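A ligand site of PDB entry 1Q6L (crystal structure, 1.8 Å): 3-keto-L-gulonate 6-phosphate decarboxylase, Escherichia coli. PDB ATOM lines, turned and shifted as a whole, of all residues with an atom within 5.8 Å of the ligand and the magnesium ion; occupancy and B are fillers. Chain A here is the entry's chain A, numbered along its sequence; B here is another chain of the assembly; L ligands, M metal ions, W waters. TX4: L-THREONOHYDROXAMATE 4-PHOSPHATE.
OD2 of Asp 11 sits close to O2 of the ligand (2.6 Å). O3 of the ligand is in hydrogen-bond range of OG1 of Thr 169 (2.6 Å). The side-chain carboxylate (OD2) of Asp 67 of chain B sits at hydrogen-bond distance from an oxygen (ON) of the ligand (2.7 Å). The backbone NH (N) of Arg 192 sits at hydrogen-bond distance from an oxygen (O5) of the ligand, 2.9 Å away. An oxygen (O5) of the ligand lies within salt-bridge range of the guanidinium group (NE) of Arg 192 (2.8 Å). The side-chain amino group (NZ) of Lys 64 is in hydrogen-bond range of an oxygen (ON) of the ligand (2.8 Å). O6 of the ligand sits at hydrogen-bond distance from N of Gly 191 (2.9 Å). O7 of the ligand sits at hydrogen-bond distance from N of Gly 171, 2.9 Å away. NE2 of His 136 lies close to N of the ligand, 3.5 Å away.
The backbone carbonyl oxygen (O) of Asp 62 lies within hydrogen-bond range of the side-chain hydroxyl (OG1) of Thr 36 (2.6 Å). The backbone carbonyl oxygen (O) of Val 34 is in hydrogen-bond range of the backbone NH (N) of Asp 62. OD2 of Asp 67 of chain B is in hydrogen-bond range of N of Arg 139 (2.9 Å). NH1 of Arg 192 is in hydrogen-bond range of OE1 of Gln 142 (3.0 Å). The side-chain hydroxyl (OG1) of Thr 36 lies within hydrogen-bond range of the side-chain amino group (NZ) of Lys 64, at 3.2 Å. The side-chain hydroxyl (OG1) of Thr 114 sits at hydrogen-bond distance from a ring nitrogen (ND1) of His 136 (2.8 Å). N of Ala 9 lies within hydrogen-bond range of O of Ala 190, at 3.2 Å. The guanidinium group (NH1) of Arg 195 sits at hydrogen-bond distance from the backbone carbonyl oxygen (O) of Ala 9 (2.8 Å).
CB of Ala 9 touches O2 of the ligand, at 3.4 Å. Gly 170 touches the ligand (C to O7, 3.9 Å). CG2 of Ile 189 touches C4 of the ligand, at 3.7 Å. Ala 190 touches the ligand. The nearest printed residue that does not touch the ligand is Leu 172 (4.03 Å).
Of the 26 residues printed, 2 come within 4 Å of the magnesium ion. The nearest printed residue that does not touch the magnesium ion is Lys 64 (4.1 Å).
The magnesium ion is bound by the side-chain carboxylate (OE2) of Glu 33 (2.0 Å), the side-chain carboxylate (OD2) of Asp 62 (2.1 Å), an oxygen (O2) of the ligand (2.1 Å), an oxygen (O1) of the ligand (2.1 Å), water W1 (2.1 Å) and water W5 (2.2 Å). The magnesium ion has six donor atoms within binding distance.
Water W1 bridges the side-chain carboxylate (OD1) of Asp 11 (2.7 Å) and the backbone NH (N) of Thr 36 (2.8 Å). Water W5 bridges O3 of the ligand (2.7 Å) and OE1 of Glu 33 (2.7 Å). Water W8 lies within hydrogen-bond range of N of the ligand (2.6 Å) and NH1 of Arg 139 (3.3 Å). Water W2 lies within hydrogen-bond range of O6 of the ligand, O of Leu 172 and N of Ser 193. Water W4 lies within hydrogen-bond range of OD2 of Asp 11 (2.7 Å), O5 of the ligand (2.8 Å) and NH1 of Arg 195 (2.8 Å). Water W6 lies within hydrogen-bond range of NZ of Lys 64 (2.9 Å), ON of the ligand (2.9 Å) and OG1 of Thr 36 (3.3 Å).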
ATOM      1  N   ALA A   9     -17.705 -23.607 -18.615  1.00  0.00           N
ATOM      2  CA  ALA A   9     -17.995 -23.562 -20.034  1.00  0.00           C
ATOM      3  C   ALA A   9     -18.434 -24.914 -20.472  1.00  0.00           C
ATOM      4  O   ALA A   9     -17.630 -25.877 -20.414  1.00  0.00           O
ATOM      5  CB  ALA A   9     -16.768 -23.108 -20.871  1.00  0.00           C
ATOM      6  N   ASP A  11     -18.657 -26.620 -23.355  1.00  0.00           N
ATOM      7  CA  ASP A  11     -18.294 -26.771 -24.757  1.00  0.00           C
ATOM      8  C   ASP A  11     -18.521 -28.196 -25.164  1.00  0.00           C
ATOM      9  O   ASP A  11     -17.564 -28.977 -25.435  1.00  0.00           O
ATOM     10  CB  ASP A  11     -16.833 -26.331 -25.001  1.00  0.00           C
ATOM     11  CG  ASP A  11     -16.687 -24.833 -24.850  1.00  0.00           C
ATOM     12  OD1 ASP A  11     -17.527 -24.168 -25.515  1.00  0.00           O
ATOM     13  OD2 ASP A  11     -15.791 -24.262 -24.174  1.00  0.00           O
ATOM     14  N   GLU A  33     -22.117 -21.540 -18.601  1.00  0.00           N
ATOM     15  CA  GLU A  33     -22.017 -21.090 -19.950  1.00  0.00           C
ATOM     16  C   GLU A  33     -22.460 -22.198 -20.936  1.00  0.00           C
ATOM     17  O   GLU A  33     -21.939 -23.357 -20.930  1.00  0.00           O
ATOM     18  CB  GLU A  33     -20.584 -20.630 -20.289  1.00  0.00           C
ATOM     19  CG  GLU A  33     -20.213 -20.741 -21.782  1.00  0.00           C
ATOM     20  CD  GLU A  33     -18.780 -20.435 -22.111  1.00  0.00           C
ATOM     21  OE1 GLU A  33     -18.046 -19.872 -21.250  1.00  0.00           O
ATOM     22  OE2 GLU A  33     -18.377 -20.793 -23.257  1.00  0.00           O
ATOM     23  N   VAL A  34     -23.357 -21.790 -21.821  1.00  0.00           N
ATOM     24  CA  VAL A  34     -23.640 -22.507 -23.049  1.00  0.00           C
ATOM     25  C   VAL A  34     -22.522 -22.152 -24.037  1.00  0.00           C
ATOM     26  O   VAL A  34     -22.501 -21.092 -24.676  1.00  0.00           O
ATOM     27  CB  VAL A  34     -24.963 -22.155 -23.628  1.00  0.00           C
ATOM     28  CG1 VAL A  34     -25.289 -23.047 -24.807  1.00  0.00           C
ATOM     29  CG2 VAL A  34     -26.021 -22.265 -22.554  1.00  0.00           C
ATOM     30  N   GLY A  35     -21.538 -23.035 -24.156  1.00  0.00           N
ATOM     31  CA  GLY A  35     -20.464 -22.674 -25.030  1.00  0.00           C
ATOM     32  C   GLY A  35     -20.856 -22.549 -26.492  1.00  0.00           C
ATOM     33  O   GLY A  35     -21.898 -23.050 -26.952  1.00  0.00           O
ATOM     34  N   THR A  36     -19.942 -21.936 -27.238  1.00  0.00           N
ATOM     35  CA  THR A  36     -20.136 -21.772 -28.663  1.00  0.00           C
ATOM     36  C   THR A  36     -20.376 -23.111 -29.343  1.00  0.00           C
ATOM     37  O   THR A  36     -21.247 -23.227 -30.175  1.00  0.00           O
ATOM     38  CB  THR A  36     -18.963 -21.051 -29.295  1.00  0.00           C
ATOM     39  OG1 THR A  36     -18.604 -19.931 -28.480  1.00  0.00           O
ATOM     40  CG2 THR A  36     -19.396 -20.440 -30.622  1.00  0.00           C
ATOM     41  N   ASP A  62     -22.687 -18.250 -25.120  1.00  0.00           N
ATOM     42  CA  ASP A  62     -21.457 -17.826 -25.731  1.00  0.00           C
ATOM     43  C   ASP A  62     -21.560 -17.896 -27.289  1.00  0.00           C
ATOM     44  O   ASP A  62     -20.771 -18.588 -27.953  1.00  0.00           O
ATOM     45  CB  ASP A  62     -20.276 -18.667 -25.158  1.00  0.00           C
ATOM     46  CG  ASP A  62     -18.934 -18.085 -25.489  1.00  0.00           C
ATOM     47  OD1 ASP A  62     -18.866 -16.886 -25.855  1.00  0.00           O
ATOM     48  OD2 ASP A  62     -17.856 -18.754 -25.419  1.00  0.00           O
ATOM     49  N   LYS A  64     -20.897 -15.451 -29.443  1.00  0.00           N
ATOM     50  CA  LYS A  64     -19.807 -14.769 -30.125  1.00  0.00           C
ATOM     51  C   LYS A  64     -20.353 -14.075 -31.355  1.00  0.00           C
ATOM     52  O   LYS A  64     -19.877 -14.196 -32.458  1.00  0.00           O
ATOM     53  CB  LYS A  64     -18.673 -15.739 -30.498  1.00  0.00           C
ATOM     54  CG  LYS A  64     -17.885 -16.146 -29.232  1.00  0.00           C
ATOM     55  CD  LYS A  64     -16.674 -17.079 -29.568  1.00  0.00           C
ATOM     56  CE  LYS A  64     -15.988 -17.398 -28.181  1.00  0.00           C
ATOM     57  NZ  LYS A  64     -15.636 -18.752 -28.058  1.00  0.00           N
ATOM     58  N   GLU A 112     -16.249 -10.227 -26.446  1.00  0.00           N
ATOM     59  CA  GLU A 112     -15.343 -11.352 -26.407  1.00  0.00           C
ATOM     60  C   GLU A 112     -14.055 -10.992 -27.117  1.00  0.00           C
ATOM     61  O   GLU A 112     -14.061 -10.796 -28.316  1.00  0.00           O
ATOM     62  CB  GLU A 112     -16.029 -12.541 -27.021  1.00  0.00           C
ATOM     63  CG  GLU A 112     -16.140 -13.707 -26.059  1.00  0.00           C
ATOM     64  CD  GLU A 112     -14.807 -14.446 -25.907  1.00  0.00           C
ATOM     65  OE1 GLU A 112     -13.826 -14.030 -26.531  1.00  0.00           O
ATOM     66  OE2 GLU A 112     -14.789 -15.466 -25.216  1.00  0.00           O
ATOM     67  N   THR A 114     -11.254 -12.309 -28.281  1.00  0.00           N
ATOM     68  CA  THR A 114     -10.540 -13.460 -28.853  1.00  0.00           C
ATOM     69  C   THR A 114     -10.009 -12.961 -30.177  1.00  0.00           C
ATOM     70  O   THR A 114     -10.769 -12.414 -30.980  1.00  0.00           O
ATOM     71  CB  THR A 114     -11.475 -14.646 -29.057  1.00  0.00           C
ATOM     72  OG1 THR A 114     -11.832 -15.206 -27.790  1.00  0.00           O
ATOM     73  CG2 THR A 114     -10.778 -15.790 -29.812  1.00  0.00           C
ATOM     74  N   VAL A 134     -14.440 -10.147 -22.095  1.00  0.00           N
ATOM     75  CA  VAL A 134     -13.817 -11.424 -21.857  1.00  0.00           C
ATOM     76  C   VAL A 134     -12.427 -11.459 -22.465  1.00  0.00           C
ATOM     77  O   VAL A 134     -12.288 -11.523 -23.690  1.00  0.00           O
ATOM     78  CB  VAL A 134     -14.651 -12.583 -22.475  1.00  0.00           C
ATOM     79  CG1 VAL A 134     -14.086 -13.935 -22.068  1.00  0.00           C
ATOM     80  CG2 VAL A 134     -16.062 -12.545 -21.976  1.00  0.00           C
ATOM     81  N   HIS A 136      -9.343 -13.301 -23.415  1.00  0.00           N
ATOM     82  CA  HIS A 136      -9.439 -14.676 -23.805  1.00  0.00           C
ATOM     83  C   HIS A 136      -8.258 -15.092 -24.649  1.00  0.00           C
ATOM     84  O   HIS A 136      -8.048 -14.611 -25.785  1.00  0.00           O
ATOM     85  CB  HIS A 136     -10.790 -14.873 -24.531  1.00  0.00           C
ATOM     86  CG  HIS A 136     -11.110 -16.294 -24.834  1.00  0.00           C
ATOM     87  ND1 HIS A 136     -12.311 -16.659 -25.401  1.00  0.00           N
ATOM     88  CD2 HIS A 136     -10.451 -17.448 -24.567  1.00  0.00           C
ATOM     89  CE1 HIS A 136     -12.327 -17.981 -25.554  1.00  0.00           C
ATOM     90  NE2 HIS A 136     -11.218 -18.494 -25.026  1.00  0.00           N
ATOM     91  N   ARG A 139      -8.312 -20.717 -27.765  1.00  0.00           N
ATOM     92  CA  ARG A 139      -7.996 -22.140 -27.737  1.00  0.00           C
ATOM     93  C   ARG A 139      -6.974 -22.555 -28.833  1.00  0.00           C
ATOM     94  O   ARG A 139      -6.081 -23.410 -28.625  1.00  0.00           O
ATOM     95  CB  ARG A 139      -9.286 -22.906 -27.958  1.00  0.00           C
ATOM     96  CG  ARG A 139      -9.095 -24.409 -28.173  1.00  0.00           C
ATOM     97  CD  ARG A 139     -10.473 -25.072 -28.360  1.00  0.00           C
ATOM     98  NE  ARG A 139     -10.410 -26.457 -27.974  1.00  0.00           N
ATOM     99  CZ  ARG A 139     -11.102 -27.048 -27.000  1.00  0.00           C
ATOM    100  NH1 ARG A 139     -11.986 -26.406 -26.252  1.00  0.00           N
ATOM    101  NH2 ARG A 139     -10.867 -28.342 -26.822  1.00  0.00           N
ATOM    102  N   GLN A 142      -3.538 -21.169 -28.034  1.00  0.00           N
ATOM    103  CA  GLN A 142      -3.020 -22.096 -27.010  1.00  0.00           C
ATOM    104  C   GLN A 142      -2.405 -23.363 -27.608  1.00  0.00           C
ATOM    105  O   GLN A 142      -1.309 -23.772 -27.238  1.00  0.00           O
ATOM    106  CB  GLN A 142      -4.106 -22.517 -26.030  1.00  0.00           C
ATOM    107  CG  GLN A 142      -3.652 -23.575 -24.989  1.00  0.00           C
ATOM    108  CD  GLN A 142      -4.724 -23.963 -24.038  1.00  0.00           C
ATOM    109  OE1 GLN A 142      -5.842 -23.365 -24.075  1.00  0.00           O
ATOM    110  NE2 GLN A 142      -4.440 -24.975 -23.192  1.00  0.00           N
ATOM    111  N   THR A 169     -10.148 -16.065 -19.313  1.00  0.00           N
ATOM    112  CA  THR A 169     -10.403 -17.433 -19.791  1.00  0.00           C
ATOM    113  C   THR A 169      -9.387 -17.812 -20.821  1.00  0.00           C
ATOM    114  O   THR A 169      -8.820 -16.969 -21.500  1.00  0.00           O
ATOM    115  CB  THR A 169     -11.850 -17.539 -20.382  1.00  0.00           C
ATOM    116  OG1 THR A 169     -12.193 -18.922 -20.644  1.00  0.00           O
ATOM    117  CG2 THR A 169     -11.958 -16.841 -21.731  1.00  0.00           C
ATOM    118  N   GLY A 170      -9.108 -19.096 -20.901  1.00  0.00           N
ATOM    119  CA  GLY A 170      -8.457 -19.606 -22.071  1.00  0.00           C
ATOM    120  C   GLY A 170      -7.554 -20.682 -21.607  1.00  0.00           C
ATOM    121  O   GLY A 170      -6.388 -20.438 -21.282  1.00  0.00           O
ATOM    122  N   GLY A 171      -8.125 -21.860 -21.478  1.00  0.00           N
ATOM    123  CA  GLY A 171      -7.371 -23.030 -21.029  1.00  0.00           C
ATOM    124  C   GLY A 171      -6.845 -22.891 -19.644  1.00  0.00           C
ATOM    125  O   GLY A 171      -5.758 -23.417 -19.285  1.00  0.00           O
ATOM    126  N   LEU A 172      -7.606 -22.194 -18.812  1.00  0.00           N
ATOM    127  CA  LEU A 172      -7.148 -21.926 -17.425  1.00  0.00           C
ATOM    128  C   LEU A 172      -7.013 -23.245 -16.627  1.00  0.00           C
ATOM    129  O   LEU A 172      -7.911 -24.084 -16.669  1.00  0.00           O
ATOM    130  CB  LEU A 172      -8.137 -21.010 -16.672  1.00  0.00           C
ATOM    131  CG  LEU A 172      -7.866 -19.539 -16.294  1.00  0.00           C
ATOM    132  CD1 LEU A 172      -6.650 -18.889 -16.923  1.00  0.00           C
ATOM    133  CD2 LEU A 172      -9.091 -18.732 -16.565  1.00  0.00           C
ATOM    134  N   ILE A 189     -13.354 -18.277 -16.210  1.00  0.00           N
ATOM    135  CA  ILE A 189     -13.979 -19.400 -16.866  1.00  0.00           C
ATOM    136  C   ILE A 189     -13.048 -20.621 -16.857  1.00  0.00           C
ATOM    137  O   ILE A 189     -11.833 -20.511 -17.142  1.00  0.00           O
ATOM    138  CB  ILE A 189     -14.319 -19.096 -18.287  1.00  0.00           C
ATOM    139  CG1 ILE A 189     -15.124 -17.801 -18.431  1.00  0.00           C
ATOM    140  CG2 ILE A 189     -15.069 -20.239 -18.874  1.00  0.00           C
ATOM    141  CD1 ILE A 189     -15.452 -17.445 -19.853  1.00  0.00           C
ATOM    142  N   ALA A 190     -13.608 -21.785 -16.539  1.00  0.00           N
ATOM    143  CA  ALA A 190     -12.930 -23.057 -16.816  1.00  0.00           C
ATOM    144  C   ALA A 190     -13.853 -23.970 -17.565  1.00  0.00           C
ATOM    145  O   ALA A 190     -14.996 -24.232 -17.075  1.00  0.00           O
ATOM    146  CB  ALA A 190     -12.525 -23.740 -15.541  1.00  0.00           C
ATOM    147  N   GLY A 191     -13.363 -24.483 -18.709  1.00  0.00           N
ATOM    148  CA  GLY A 191     -14.068 -25.487 -19.498  1.00  0.00           C
ATOM    149  C   GLY A 191     -13.403 -26.854 -19.306  1.00  0.00           C
ATOM    150  O   GLY A 191     -13.769 -27.656 -18.450  1.00  0.00           O
ATOM    151  N   ARG A 192     -12.337 -27.071 -20.022  1.00  0.00           N
ATOM    152  CA  ARG A 192     -11.668 -28.386 -19.994  1.00  0.00           C
ATOM    153  C   ARG A 192     -11.162 -28.818 -18.613  1.00  0.00           C
ATOM    154  O   ARG A 192     -11.215 -30.015 -18.254  1.00  0.00           O
ATOM    155  CB  ARG A 192     -10.511 -28.313 -20.979  1.00  0.00           C
ATOM    156  CG  ARG A 192     -10.948 -28.423 -22.370  1.00  0.00           C
ATOM    157  CD  ARG A 192      -9.837 -28.061 -23.356  1.00  0.00           C
ATOM    158  NE  ARG A 192      -9.673 -26.612 -23.424  1.00  0.00           N
ATOM    159  CZ  ARG A 192      -8.598 -25.995 -23.927  1.00  0.00           C
ATOM    160  NH1 ARG A 192      -8.577 -24.672 -23.967  1.00  0.00           N
ATOM    161  NH2 ARG A 192      -7.566 -26.686 -24.432  1.00  0.00           N
ATOM    162  N   SER A 193     -10.554 -27.888 -17.900  1.00  0.00           N
ATOM    163  CA  SER A 193      -9.968 -28.148 -16.583  1.00  0.00           C
ATOM    164  C   SER A 193     -11.037 -28.572 -15.516  1.00  0.00           C
ATOM    165  O   SER A 193     -10.693 -29.202 -14.501  1.00  0.00           O
ATOM    166  CB  SER A 193      -9.092 -26.944 -16.136  1.00  0.00           C
ATOM    167  OG  SER A 193      -9.904 -25.833 -15.670  1.00  0.00           O
ATOM    168  N   ARG A 195     -14.522 -29.937 -16.843  1.00  0.00           N
ATOM    169  CA  ARG A 195     -15.269 -31.016 -17.525  1.00  0.00           C
ATOM    170  C   ARG A 195     -14.425 -32.277 -17.642  1.00  0.00           C
ATOM    171  O   ARG A 195     -14.919 -33.398 -17.512  1.00  0.00           O
ATOM    172  CB  ARG A 195     -15.650 -30.601 -18.935  1.00  0.00           C
ATOM    173  CG  ARG A 195     -16.639 -29.408 -19.006  1.00  0.00           C
ATOM    174  CD  ARG A 195     -17.411 -29.376 -20.317  1.00  0.00           C
ATOM    175  NE  ARG A 195     -16.471 -29.624 -21.388  1.00  0.00           N
ATOM    176  CZ  ARG A 195     -15.658 -28.740 -21.958  1.00  0.00           C
ATOM    177  NH1 ARG A 195     -15.725 -27.484 -21.660  1.00  0.00           N
ATOM    178  NH2 ARG A 195     -14.781 -29.159 -22.886  1.00  0.00           N
ATOM    179  N   ASP B  67     -13.174 -19.157 -32.953  1.00  0.00           N
ATOM    180  CA  ASP B  67     -12.190 -19.901 -32.130  1.00  0.00           C
ATOM    181  C   ASP B  67     -12.614 -21.342 -32.200  1.00  0.00           C
ATOM    182  O   ASP B  67     -13.692 -21.709 -32.672  1.00  0.00           O
ATOM    183  CB  ASP B  67     -12.191 -19.383 -30.676  1.00  0.00           C
ATOM    184  CG  ASP B  67     -10.976 -19.868 -29.863  1.00  0.00           C
ATOM    185  OD1 ASP B  67      -9.952 -20.370 -30.452  1.00  0.00           O
ATOM    186  OD2 ASP B  67     -10.950 -19.801 -28.641  1.00  0.00           O
ATOM    187  N   ALA B  68     -11.760 -22.231 -31.730  1.00  0.00           N
ATOM    188  CA  ALA B  68     -12.080 -23.618 -31.796  1.00  0.00           C
ATOM    189  C   ALA B  68     -12.354 -24.055 -33.277  1.00  0.00           C
ATOM    190  O   ALA B  68     -13.274 -24.806 -33.580  1.00  0.00           O
ATOM    191  CB  ALA B  68     -13.200 -23.968 -30.839  1.00  0.00           C
HETATM  192  O7  TX4 L   1     -10.526 -22.991 -22.670  1.00  0.00           O
HETATM  193  P   TX4 L   1     -11.472 -23.718 -21.711  1.00  0.00           P
HETATM  194  O5  TX4 L   1     -11.622 -25.156 -22.110  1.00  0.00           O
HETATM  195  O6  TX4 L   1     -11.170 -23.417 -20.253  1.00  0.00           O
HETATM  196  O4  TX4 L   1     -12.948 -23.139 -22.073  1.00  0.00           O
HETATM  197  C4  TX4 L   1     -13.273 -21.794 -21.764  1.00  0.00           C
HETATM  198  C3  TX4 L   1     -13.243 -21.004 -23.068  1.00  0.00           C
HETATM  199  O3  TX4 L   1     -13.611 -19.632 -22.746  1.00  0.00           O
HETATM  200  C2  TX4 L   1     -14.144 -21.654 -24.128  1.00  0.00           C
HETATM  201  O2  TX4 L   1     -15.522 -21.754 -23.748  1.00  0.00           O
HETATM  202  C1  TX4 L   1     -14.104 -20.839 -25.378  1.00  0.00           C
HETATM  203  O1  TX4 L   1     -15.045 -19.923 -25.562  1.00  0.00           O
HETATM  204  N   TX4 L   1     -13.239 -21.060 -26.248  1.00  0.00           N
HETATM  205  ON  TX4 L   1     -13.342 -20.211 -27.370  1.00  0.00           O
HETATM  206 MG    MG M   1     -16.815 -20.260 -24.451  1.00  0.00          MG
HETATM  207  O   HOH W   1     -17.404 -21.566 -26.016  1.00  0.00           O
HETATM  208  O   HOH W   2      -9.639 -25.124 -18.909  1.00  0.00           O
HETATM  209  O   HOH W   3     -10.109 -21.181 -24.791  1.00  0.00           O
HETATM  210  O   HOH W   4     -13.962 -25.999 -23.296  1.00  0.00           O
HETATM  211  O   HOH W   5     -16.200 -18.765 -22.954  1.00  0.00           O
HETATM  212  O   HOH W   6     -15.728 -21.611 -28.322  1.00  0.00           O
HETATM  213  O   HOH W   7     -10.253 -21.266 -19.245  1.00  0.00           O
HETATM  214  O   HOH W   8     -11.737 -23.162 -25.738  1.00  0.00           O
